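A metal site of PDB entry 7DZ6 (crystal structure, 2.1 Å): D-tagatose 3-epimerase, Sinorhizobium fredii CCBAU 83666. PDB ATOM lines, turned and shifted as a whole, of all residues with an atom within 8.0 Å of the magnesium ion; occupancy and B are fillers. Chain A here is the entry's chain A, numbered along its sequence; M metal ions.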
ATOM      1  N   HIS A   9       8.435   1.307  -2.694  1.00  0.00           N
ATOM      2  CA  HIS A   9       8.725   1.632  -1.309  1.00  0.00           C
ATOM      3  C   HIS A   9       9.447   2.962  -1.238  1.00  0.00           C
ATOM      4  O   HIS A   9      10.503   3.127  -1.856  1.00  0.00           O
ATOM      5  CB  HIS A   9       9.573   0.511  -0.723  1.00  0.00           C
ATOM      6  CG  HIS A   9       9.643   0.508   0.759  1.00  0.00           C
ATOM      7  ND1 HIS A   9      10.519   1.298   1.459  1.00  0.00           N
ATOM      8  CD2 HIS A   9       8.978  -0.229   1.679  1.00  0.00           C
ATOM      9  CE1 HIS A   9      10.385   1.058   2.747  1.00  0.00           C
ATOM     10  NE2 HIS A   9       9.463   0.124   2.909  1.00  0.00           N
ATOM     11  N   GLU A  38       4.378   2.645  -1.033  1.00  0.00           N
ATOM     12  CA  GLU A  38       4.405   2.029   0.274  1.00  0.00           C
ATOM     13  C   GLU A  38       5.103   3.005   1.201  1.00  0.00           C
ATOM     14  O   GLU A  38       6.267   3.362   0.958  1.00  0.00           O
ATOM     15  CB  GLU A  38       5.119   0.683   0.257  1.00  0.00           C
ATOM     16  CG  GLU A  38       5.124  -0.044   1.599  1.00  0.00           C
ATOM     17  CD  GLU A  38       5.901  -1.383   1.549  1.00  0.00           C
ATOM     18  OE1 GLU A  38       5.977  -2.016   0.468  1.00  0.00           O
ATOM     19  OE2 GLU A  38       6.439  -1.811   2.590  1.00  0.00           O
ATOM     20  N   SER A  66       3.919   0.234   5.895  1.00  0.00           N
ATOM     21  CA  SER A  66       4.578  -0.899   6.525  1.00  0.00           C
ATOM     22  C   SER A  66       5.355  -0.424   7.738  1.00  0.00           C
ATOM     23  O   SER A  66       5.744   0.737   7.835  1.00  0.00           O
ATOM     24  CB  SER A  66       5.519  -1.615   5.519  1.00  0.00           C
ATOM     25  OG  SER A  66       6.430  -0.699   4.940  1.00  0.00           O
ATOM     26  N   GLY A 103       4.072  -5.649   6.581  1.00  0.00           N
ATOM     27  CA  GLY A 103       5.432  -5.662   7.076  1.00  0.00           C
ATOM     28  C   GLY A 103       5.582  -6.601   8.243  1.00  0.00           C
ATOM     29  O   GLY A 103       4.831  -7.584   8.378  1.00  0.00           O
ATOM     30  N   VAL A 104       6.565  -6.324   9.074  1.00  0.00           N
ATOM     31  CA  VAL A 104       6.853  -7.245  10.180  1.00  0.00           C
ATOM     32  C   VAL A 104       5.977  -6.766  11.348  1.00  0.00           C
ATOM     33  O   VAL A 104       6.469  -6.168  12.306  1.00  0.00           O
ATOM     34  CB  VAL A 104       8.356  -7.300  10.508  1.00  0.00           C
ATOM     35  CG1 VAL A 104       8.593  -8.368  11.558  1.00  0.00           C
ATOM     36  CG2 VAL A 104       9.186  -7.617   9.249  1.00  0.00           C
ATOM     37  N   ILE A 109      12.407  -6.347  13.665  1.00  0.00           N
ATOM     38  CA  ILE A 109      13.676  -6.552  12.990  1.00  0.00           C
ATOM     39  C   ILE A 109      14.762  -6.629  14.052  1.00  0.00           C
ATOM     40  O   ILE A 109      14.931  -5.692  14.853  1.00  0.00           O
ATOM     41  CB  ILE A 109      13.938  -5.450  11.948  1.00  0.00           C
ATOM     42  CG1 ILE A 109      12.723  -5.336  11.012  1.00  0.00           C
ATOM     43  CG2 ILE A 109      15.283  -5.674  11.248  1.00  0.00           C
ATOM     44  CD1 ILE A 109      12.736  -6.229   9.708  1.00  0.00           C
ATOM     45  N   GLU A 146       4.545 -10.109   6.652  1.00  0.00           N
ATOM     46  CA  GLU A 146       5.678 -10.258   5.739  1.00  0.00           C
ATOM     47  C   GLU A 146       6.625 -11.320   6.271  1.00  0.00           C
ATOM     48  O   GLU A 146       7.137 -11.205   7.384  1.00  0.00           O
ATOM     49  CB  GLU A 146       6.408  -8.921   5.581  1.00  0.00           C
ATOM     50  CG  GLU A 146       7.523  -8.972   4.524  1.00  0.00           C
ATOM     51  CD  GLU A 146       8.340  -7.687   4.391  1.00  0.00           C
ATOM     52  OE1 GLU A 146       8.176  -6.735   5.204  1.00  0.00           O
ATOM     53  OE2 GLU A 146       9.174  -7.661   3.461  1.00  0.00           O
ATOM     54  N   ALA A 147       6.839 -12.375   5.479  1.00  0.00           N
ATOM     55  CA  ALA A 147       7.914 -13.313   5.773  1.00  0.00           C
ATOM     56  C   ALA A 147       9.266 -12.630   5.585  1.00  0.00           C
ATOM     57  O   ALA A 147       9.519 -12.056   4.514  1.00  0.00           O
ATOM     58  CB  ALA A 147       7.812 -14.539   4.853  1.00  0.00           C
ATOM     59  N   VAL A 148      10.126 -12.665   6.606  1.00  0.00           N
ATOM     60  CA  VAL A 148      11.475 -12.093   6.491  1.00  0.00           C
ATOM     61  C   VAL A 148      12.512 -13.150   6.856  1.00  0.00           C
ATOM     62  O   VAL A 148      12.169 -14.209   7.371  1.00  0.00           O
ATOM     63  CB  VAL A 148      11.671 -10.834   7.399  1.00  0.00           C
ATOM     64  CG1 VAL A 148      10.664  -9.743   7.002  1.00  0.00           C
ATOM     65  CG2 VAL A 148      11.582 -11.204   8.848  1.00  0.00           C
ATOM     66  N   GLU A 152      16.553 -11.642  10.588  1.00  0.00           N
ATOM     67  CA  GLU A 152      15.796 -10.470  10.991  1.00  0.00           C
ATOM     68  C   GLU A 152      14.757 -10.829  12.026  1.00  0.00           C
ATOM     69  O   GLU A 152      14.403  -9.988  12.864  1.00  0.00           O
ATOM     70  CB  GLU A 152      15.136  -9.839   9.760  1.00  0.00           C
ATOM     71  CG  GLU A 152      16.200  -9.279   8.813  1.00  0.00           C
ATOM     72  CD  GLU A 152      15.673  -8.288   7.755  1.00  0.00           C
ATOM     73  OE1 GLU A 152      14.441  -8.015   7.724  1.00  0.00           O
ATOM     74  OE2 GLU A 152      16.515  -7.832   6.931  1.00  0.00           O
ATOM     75  N   HIS A 177       2.564 -11.350   2.652  1.00  0.00           N
ATOM     76  CA  HIS A 177       3.411 -10.347   2.019  1.00  0.00           C
ATOM     77  C   HIS A 177       4.752 -11.015   1.858  1.00  0.00           C
ATOM     78  O   HIS A 177       5.366 -11.356   2.866  1.00  0.00           O
ATOM     79  CB  HIS A 177       3.470  -9.084   2.891  1.00  0.00           C
ATOM     80  CG  HIS A 177       4.460  -8.044   2.454  1.00  0.00           C
ATOM     81  ND1 HIS A 177       4.392  -6.736   2.892  1.00  0.00           N
ATOM     82  CD2 HIS A 177       5.576  -8.124   1.695  1.00  0.00           C
ATOM     83  CE1 HIS A 177       5.399  -6.054   2.396  1.00  0.00           C
ATOM     84  NE2 HIS A 177       6.139  -6.870   1.660  1.00  0.00           N
ATOM     85  N   LEU A 178       5.185 -11.217   0.611  1.00  0.00           N
ATOM     86  CA  LEU A 178       6.445 -11.892   0.343  1.00  0.00           C
ATOM     87  C   LEU A 178       7.446 -10.861  -0.118  1.00  0.00           C
ATOM     88  O   LEU A 178       7.078  -9.789  -0.580  1.00  0.00           O
ATOM     89  CB  LEU A 178       6.293 -12.984  -0.701  1.00  0.00           C
ATOM     90  CG  LEU A 178       5.507 -14.232  -0.233  1.00  0.00           C
ATOM     91  CD1 LEU A 178       5.295 -15.242  -1.417  1.00  0.00           C
ATOM     92  CD2 LEU A 178       6.191 -14.900   0.932  1.00  0.00           C
ATOM     93  N   ASP A 179       8.730 -11.225  -0.013  1.00  0.00           N
ATOM     94  CA  ASP A 179       9.825 -10.367  -0.448  1.00  0.00           C
ATOM     95  C   ASP A 179      10.895 -11.254  -1.077  1.00  0.00           C
ATOM     96  O   ASP A 179      11.353 -12.220  -0.444  1.00  0.00           O
ATOM     97  CB  ASP A 179      10.391  -9.541   0.733  1.00  0.00           C
ATOM     98  CG  ASP A 179      11.549  -8.631   0.314  1.00  0.00           C
ATOM     99  OD1 ASP A 179      12.287  -8.965  -0.683  1.00  0.00           O
ATOM    100  OD2 ASP A 179      11.752  -7.571   0.983  1.00  0.00           O
ATOM    101  N   THR A 180      11.287 -10.931  -2.308  1.00  0.00           N
ATOM    102  CA  THR A 180      12.158 -11.800  -3.089  1.00  0.00           C
ATOM    103  C   THR A 180      13.572 -11.838  -2.520  1.00  0.00           C
ATOM    104  O   THR A 180      14.282 -12.844  -2.646  1.00  0.00           O
ATOM    105  CB  THR A 180      12.188 -11.326  -4.554  1.00  0.00           C
ATOM    106  OG1 THR A 180      12.598  -9.947  -4.598  1.00  0.00           O
ATOM    107  CG2 THR A 180      10.823 -11.416  -5.175  1.00  0.00           C
ATOM    108  N   TYR A 181      13.957 -10.752  -1.839  1.00  0.00           N
ATOM    109  CA  TYR A 181      15.214 -10.698  -1.113  1.00  0.00           C
ATOM    110  C   TYR A 181      15.236 -11.732   0.019  1.00  0.00           C
ATOM    111  O   TYR A 181      16.198 -12.488   0.168  1.00  0.00           O
ATOM    112  CB  TYR A 181      15.434  -9.264  -0.582  1.00  0.00           C
ATOM    113  CG  TYR A 181      16.493  -9.134   0.479  1.00  0.00           C
ATOM    114  CD1 TYR A 181      17.798  -8.939   0.147  1.00  0.00           C
ATOM    115  CD2 TYR A 181      16.162  -9.234   1.831  1.00  0.00           C
ATOM    116  CE1 TYR A 181      18.760  -8.857   1.070  1.00  0.00           C
ATOM    117  CE2 TYR A 181      17.109  -9.115   2.790  1.00  0.00           C
ATOM    118  CZ  TYR A 181      18.413  -8.911   2.405  1.00  0.00           C
ATOM    119  OH  TYR A 181      19.371  -8.802   3.315  1.00  0.00           O
ATOM    120  N   HIS A 182      14.164 -11.774   0.811  1.00  0.00           N
ATOM    121  CA  HIS A 182      14.067 -12.782   1.872  1.00  0.00           C
ATOM    122  C   HIS A 182      13.877 -14.173   1.280  1.00  0.00           C
ATOM    123  O   HIS A 182      14.380 -15.163   1.819  1.00  0.00           O
ATOM    124  CB  HIS A 182      12.921 -12.445   2.812  1.00  0.00           C
ATOM    125  CG  HIS A 182      13.141 -11.170   3.577  1.00  0.00           C
ATOM    126  ND1 HIS A 182      14.321 -10.904   4.237  1.00  0.00           N
ATOM    127  CD2 HIS A 182      12.366 -10.076   3.723  1.00  0.00           C
ATOM    128  CE1 HIS A 182      14.253  -9.694   4.778  1.00  0.00           C
ATOM    129  NE2 HIS A 182      13.075  -9.187   4.508  1.00  0.00           N
ATOM    130  N   TYR A 203       0.686  -9.261  -1.906  1.00  0.00           N
ATOM    131  CA  TYR A 203       1.665  -8.209  -2.049  1.00  0.00           C
ATOM    132  C   TYR A 203       3.037  -8.818  -2.097  1.00  0.00           C
ATOM    133  O   TYR A 203       3.316  -9.742  -1.329  1.00  0.00           O
ATOM    134  CB  TYR A 203       1.578  -7.252  -0.845  1.00  0.00           C
ATOM    135  CG  TYR A 203       2.263  -5.945  -0.978  1.00  0.00           C
ATOM    136  CD1 TYR A 203       1.704  -4.923  -1.718  1.00  0.00           C
ATOM    137  CD2 TYR A 203       3.468  -5.716  -0.334  1.00  0.00           C
ATOM    138  CE1 TYR A 203       2.346  -3.677  -1.822  1.00  0.00           C
ATOM    139  CE2 TYR A 203       4.109  -4.491  -0.414  1.00  0.00           C
ATOM    140  CZ  TYR A 203       3.542  -3.479  -1.170  1.00  0.00           C
ATOM    141  OH  TYR A 203       4.182  -2.246  -1.253  1.00  0.00           O
ATOM    142  N   ILE A 204       3.911  -8.261  -2.930  1.00  0.00           N
ATOM    143  CA  ILE A 204       5.274  -8.771  -2.978  1.00  0.00           C
ATOM    144  C   ILE A 204       6.229  -7.630  -3.257  1.00  0.00           C
ATOM    145  O   ILE A 204       6.006  -6.817  -4.162  1.00  0.00           O
ATOM    146  CB  ILE A 204       5.395  -9.916  -4.022  1.00  0.00           C
ATOM    147  CG1 ILE A 204       6.789 -10.552  -3.967  1.00  0.00           C
ATOM    148  CG2 ILE A 204       5.064  -9.457  -5.410  1.00  0.00           C
ATOM    149  CD1 ILE A 204       6.945 -11.795  -4.973  1.00  0.00           C
ATOM    150  N   HIS A 205       7.301  -7.575  -2.457  1.00  0.00           N
ATOM    151  CA  HIS A 205       8.460  -6.747  -2.696  1.00  0.00           C
ATOM    152  C   HIS A 205       9.365  -7.396  -3.735  1.00  0.00           C
ATOM    153  O   HIS A 205       9.860  -8.519  -3.526  1.00  0.00           O
ATOM    154  CB  HIS A 205       9.282  -6.533  -1.436  1.00  0.00           C
ATOM    155  CG  HIS A 205       8.706  -5.559  -0.468  1.00  0.00           C
ATOM    156  ND1 HIS A 205       9.101  -5.502   0.854  1.00  0.00           N
ATOM    157  CD2 HIS A 205       7.779  -4.589  -0.628  1.00  0.00           C
ATOM    158  CE1 HIS A 205       8.435  -4.537   1.474  1.00  0.00           C
ATOM    159  NE2 HIS A 205       7.631  -3.961   0.587  1.00  0.00           N
ATOM    160  N   LEU A 206       9.649  -6.657  -4.799  1.00  0.00           N
ATOM    161  CA  LEU A 206      10.578  -7.074  -5.828  1.00  0.00           C
ATOM    162  C   LEU A 206      11.881  -6.367  -5.490  1.00  0.00           C
ATOM    163  O   LEU A 206      12.133  -5.228  -5.896  1.00  0.00           O
ATOM    164  CB  LEU A 206      10.066  -6.748  -7.219  1.00  0.00           C
ATOM    165  CG  LEU A 206       8.654  -7.321  -7.443  1.00  0.00           C
ATOM    166  CD1 LEU A 206       8.081  -6.697  -8.698  1.00  0.00           C
ATOM    167  CD2 LEU A 206       8.685  -8.862  -7.553  1.00  0.00           C
ATOM    168  N   SER A 207      12.692  -7.034  -4.729  1.00  0.00           N
ATOM    169  CA  SER A 207      13.964  -6.513  -4.276  1.00  0.00           C
ATOM    170  C   SER A 207      15.017  -7.514  -4.687  1.00  0.00           C
ATOM    171  O   SER A 207      14.826  -8.716  -4.632  1.00  0.00           O
ATOM    172  CB  SER A 207      13.912  -6.257  -2.718  1.00  0.00           C
ATOM    173  OG  SER A 207      15.211  -6.049  -2.205  1.00  0.00           O
ATOM    174  N   ARG A 211      19.700  -6.020  -2.020  1.00  0.00           N
ATOM    175  CA  ARG A 211      18.923  -4.810  -1.888  1.00  0.00           C
ATOM    176  C   ARG A 211      19.337  -3.726  -2.880  1.00  0.00           C
ATOM    177  O   ARG A 211      18.989  -2.551  -2.695  1.00  0.00           O
ATOM    178  CB  ARG A 211      18.951  -4.258  -0.443  1.00  0.00           C
ATOM    179  CG  ARG A 211      18.389  -5.198   0.675  1.00  0.00           C
ATOM    180  CD  ARG A 211      16.906  -5.496   0.469  1.00  0.00           C
ATOM    181  NE  ARG A 211      16.238  -5.953   1.681  1.00  0.00           N
ATOM    182  CZ  ARG A 211      14.945  -6.268   1.753  1.00  0.00           C
ATOM    183  NH1 ARG A 211      14.177  -6.191   0.690  1.00  0.00           N
ATOM    184  NH2 ARG A 211      14.406  -6.663   2.907  1.00  0.00           N
ATOM    185  N   ALA A 238       5.833  -4.310  -5.743  1.00  0.00           N
ATOM    186  CA  ALA A 238       6.467  -3.121  -5.173  1.00  0.00           C
ATOM    187  C   ALA A 238       7.971  -3.264  -5.179  1.00  0.00           C
ATOM    188  O   ALA A 238       8.522  -4.156  -4.518  1.00  0.00           O
ATOM    189  CB  ALA A 238       5.960  -2.861  -3.750  1.00  0.00           C
ATOM    190  N   GLU A 240      11.547  -2.518  -3.902  1.00  0.00           N
ATOM    191  CA  GLU A 240      12.206  -2.094  -2.681  1.00  0.00           C
ATOM    192  C   GLU A 240      13.712  -2.172  -2.932  1.00  0.00           C
ATOM    193  O   GLU A 240      14.241  -3.238  -3.287  1.00  0.00           O
ATOM    194  CB  GLU A 240      11.801  -2.971  -1.485  1.00  0.00           C
ATOM    195  CG  GLU A 240      12.211  -2.399  -0.118  1.00  0.00           C
ATOM    196  CD  GLU A 240      11.858  -3.314   1.049  1.00  0.00           C
ATOM    197  OE1 GLU A 240      11.807  -4.540   0.806  1.00  0.00           O
ATOM    198  OE2 GLU A 240      11.624  -2.818   2.204  1.00  0.00           O
ATOM    199  N   PHE A 242      17.315  -0.320  -0.918  1.00  0.00           N
ATOM    200  CA  PHE A 242      17.704   0.505   0.211  1.00  0.00           C
ATOM    201  C   PHE A 242      18.617   1.651  -0.211  1.00  0.00           C
ATOM    202  O   PHE A 242      19.213   2.303   0.657  1.00  0.00           O
ATOM    203  CB  PHE A 242      18.356  -0.342   1.316  1.00  0.00           C
ATOM    204  CG  PHE A 242      17.393  -1.305   2.006  1.00  0.00           C
ATOM    205  CD1 PHE A 242      16.013  -1.117   1.942  1.00  0.00           C
ATOM    206  CD2 PHE A 242      17.874  -2.396   2.721  1.00  0.00           C
ATOM    207  CE1 PHE A 242      15.138  -2.012   2.554  1.00  0.00           C
ATOM    208  CE2 PHE A 242      17.003  -3.287   3.341  1.00  0.00           C
ATOM    209  CZ  PHE A 242      15.630  -3.090   3.245  1.00  0.00           C
ATOM    210  N   LEU A 253      19.207  -2.634   9.428  1.00  0.00           N
ATOM    211  CA  LEU A 253      18.909  -3.752   8.526  1.00  0.00           C
ATOM    212  C   LEU A 253      20.153  -4.384   7.924  1.00  0.00           C
ATOM    213  O   LEU A 253      20.058  -5.128   6.934  1.00  0.00           O
ATOM    214  CB  LEU A 253      18.018  -3.278   7.379  1.00  0.00           C
ATOM    215  CG  LEU A 253      16.583  -2.902   7.718  1.00  0.00           C
ATOM    216  CD1 LEU A 253      16.225  -1.604   7.017  1.00  0.00           C
ATOM    217  CD2 LEU A 253      15.688  -4.055   7.299  1.00  0.00           C
HETATM  218 MG    MG M   1      10.382  -6.365   2.291  1.00  0.00          MG
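Within 4 Å of the magnesium ion: Glu 146, Asp 179, His 205 and Glu 240. The nearest printed residue that does not touch the magnesium ion is Arg 211 (4.1 Å).
ND1 of His 205 sits close to OE1 of Glu 240 (2.9 Å). OE1 of Glu 38 lies within hydrogen-bond range of NE2 of His 205. The backbone carbonyl oxygen of Gly 103 is in hydrogen-bond range of the backbone NH of Glu 146, at 3.1 Å. NH1 of Arg 211 lies within salt-bridge range of OD1 of Asp 179 (3.6 Å). The backbone NH (N) of Tyr 181 sits at hydrogen-bond distance from the side-chain carboxylate (OD1) of Asp 179, at 2.7 Å. OE1 of Glu 240 is in salt-bridge range of NH1 of Arg 211 (2.9 Å). OG of Ser 207 lies close to O of Glu 240 (3.2 Å). N of Glu 240 is in hydrogen-bond range of O of Leu 206 (3.4 Å).
The magnesium ion is bound by ND1 of His 205, OE2 of Glu 146 and OD2 of Asp 179. Slightly farther from the magnesium ion lies the side-chain carboxylate (OE1) of Glu 240 (2.8 Å).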
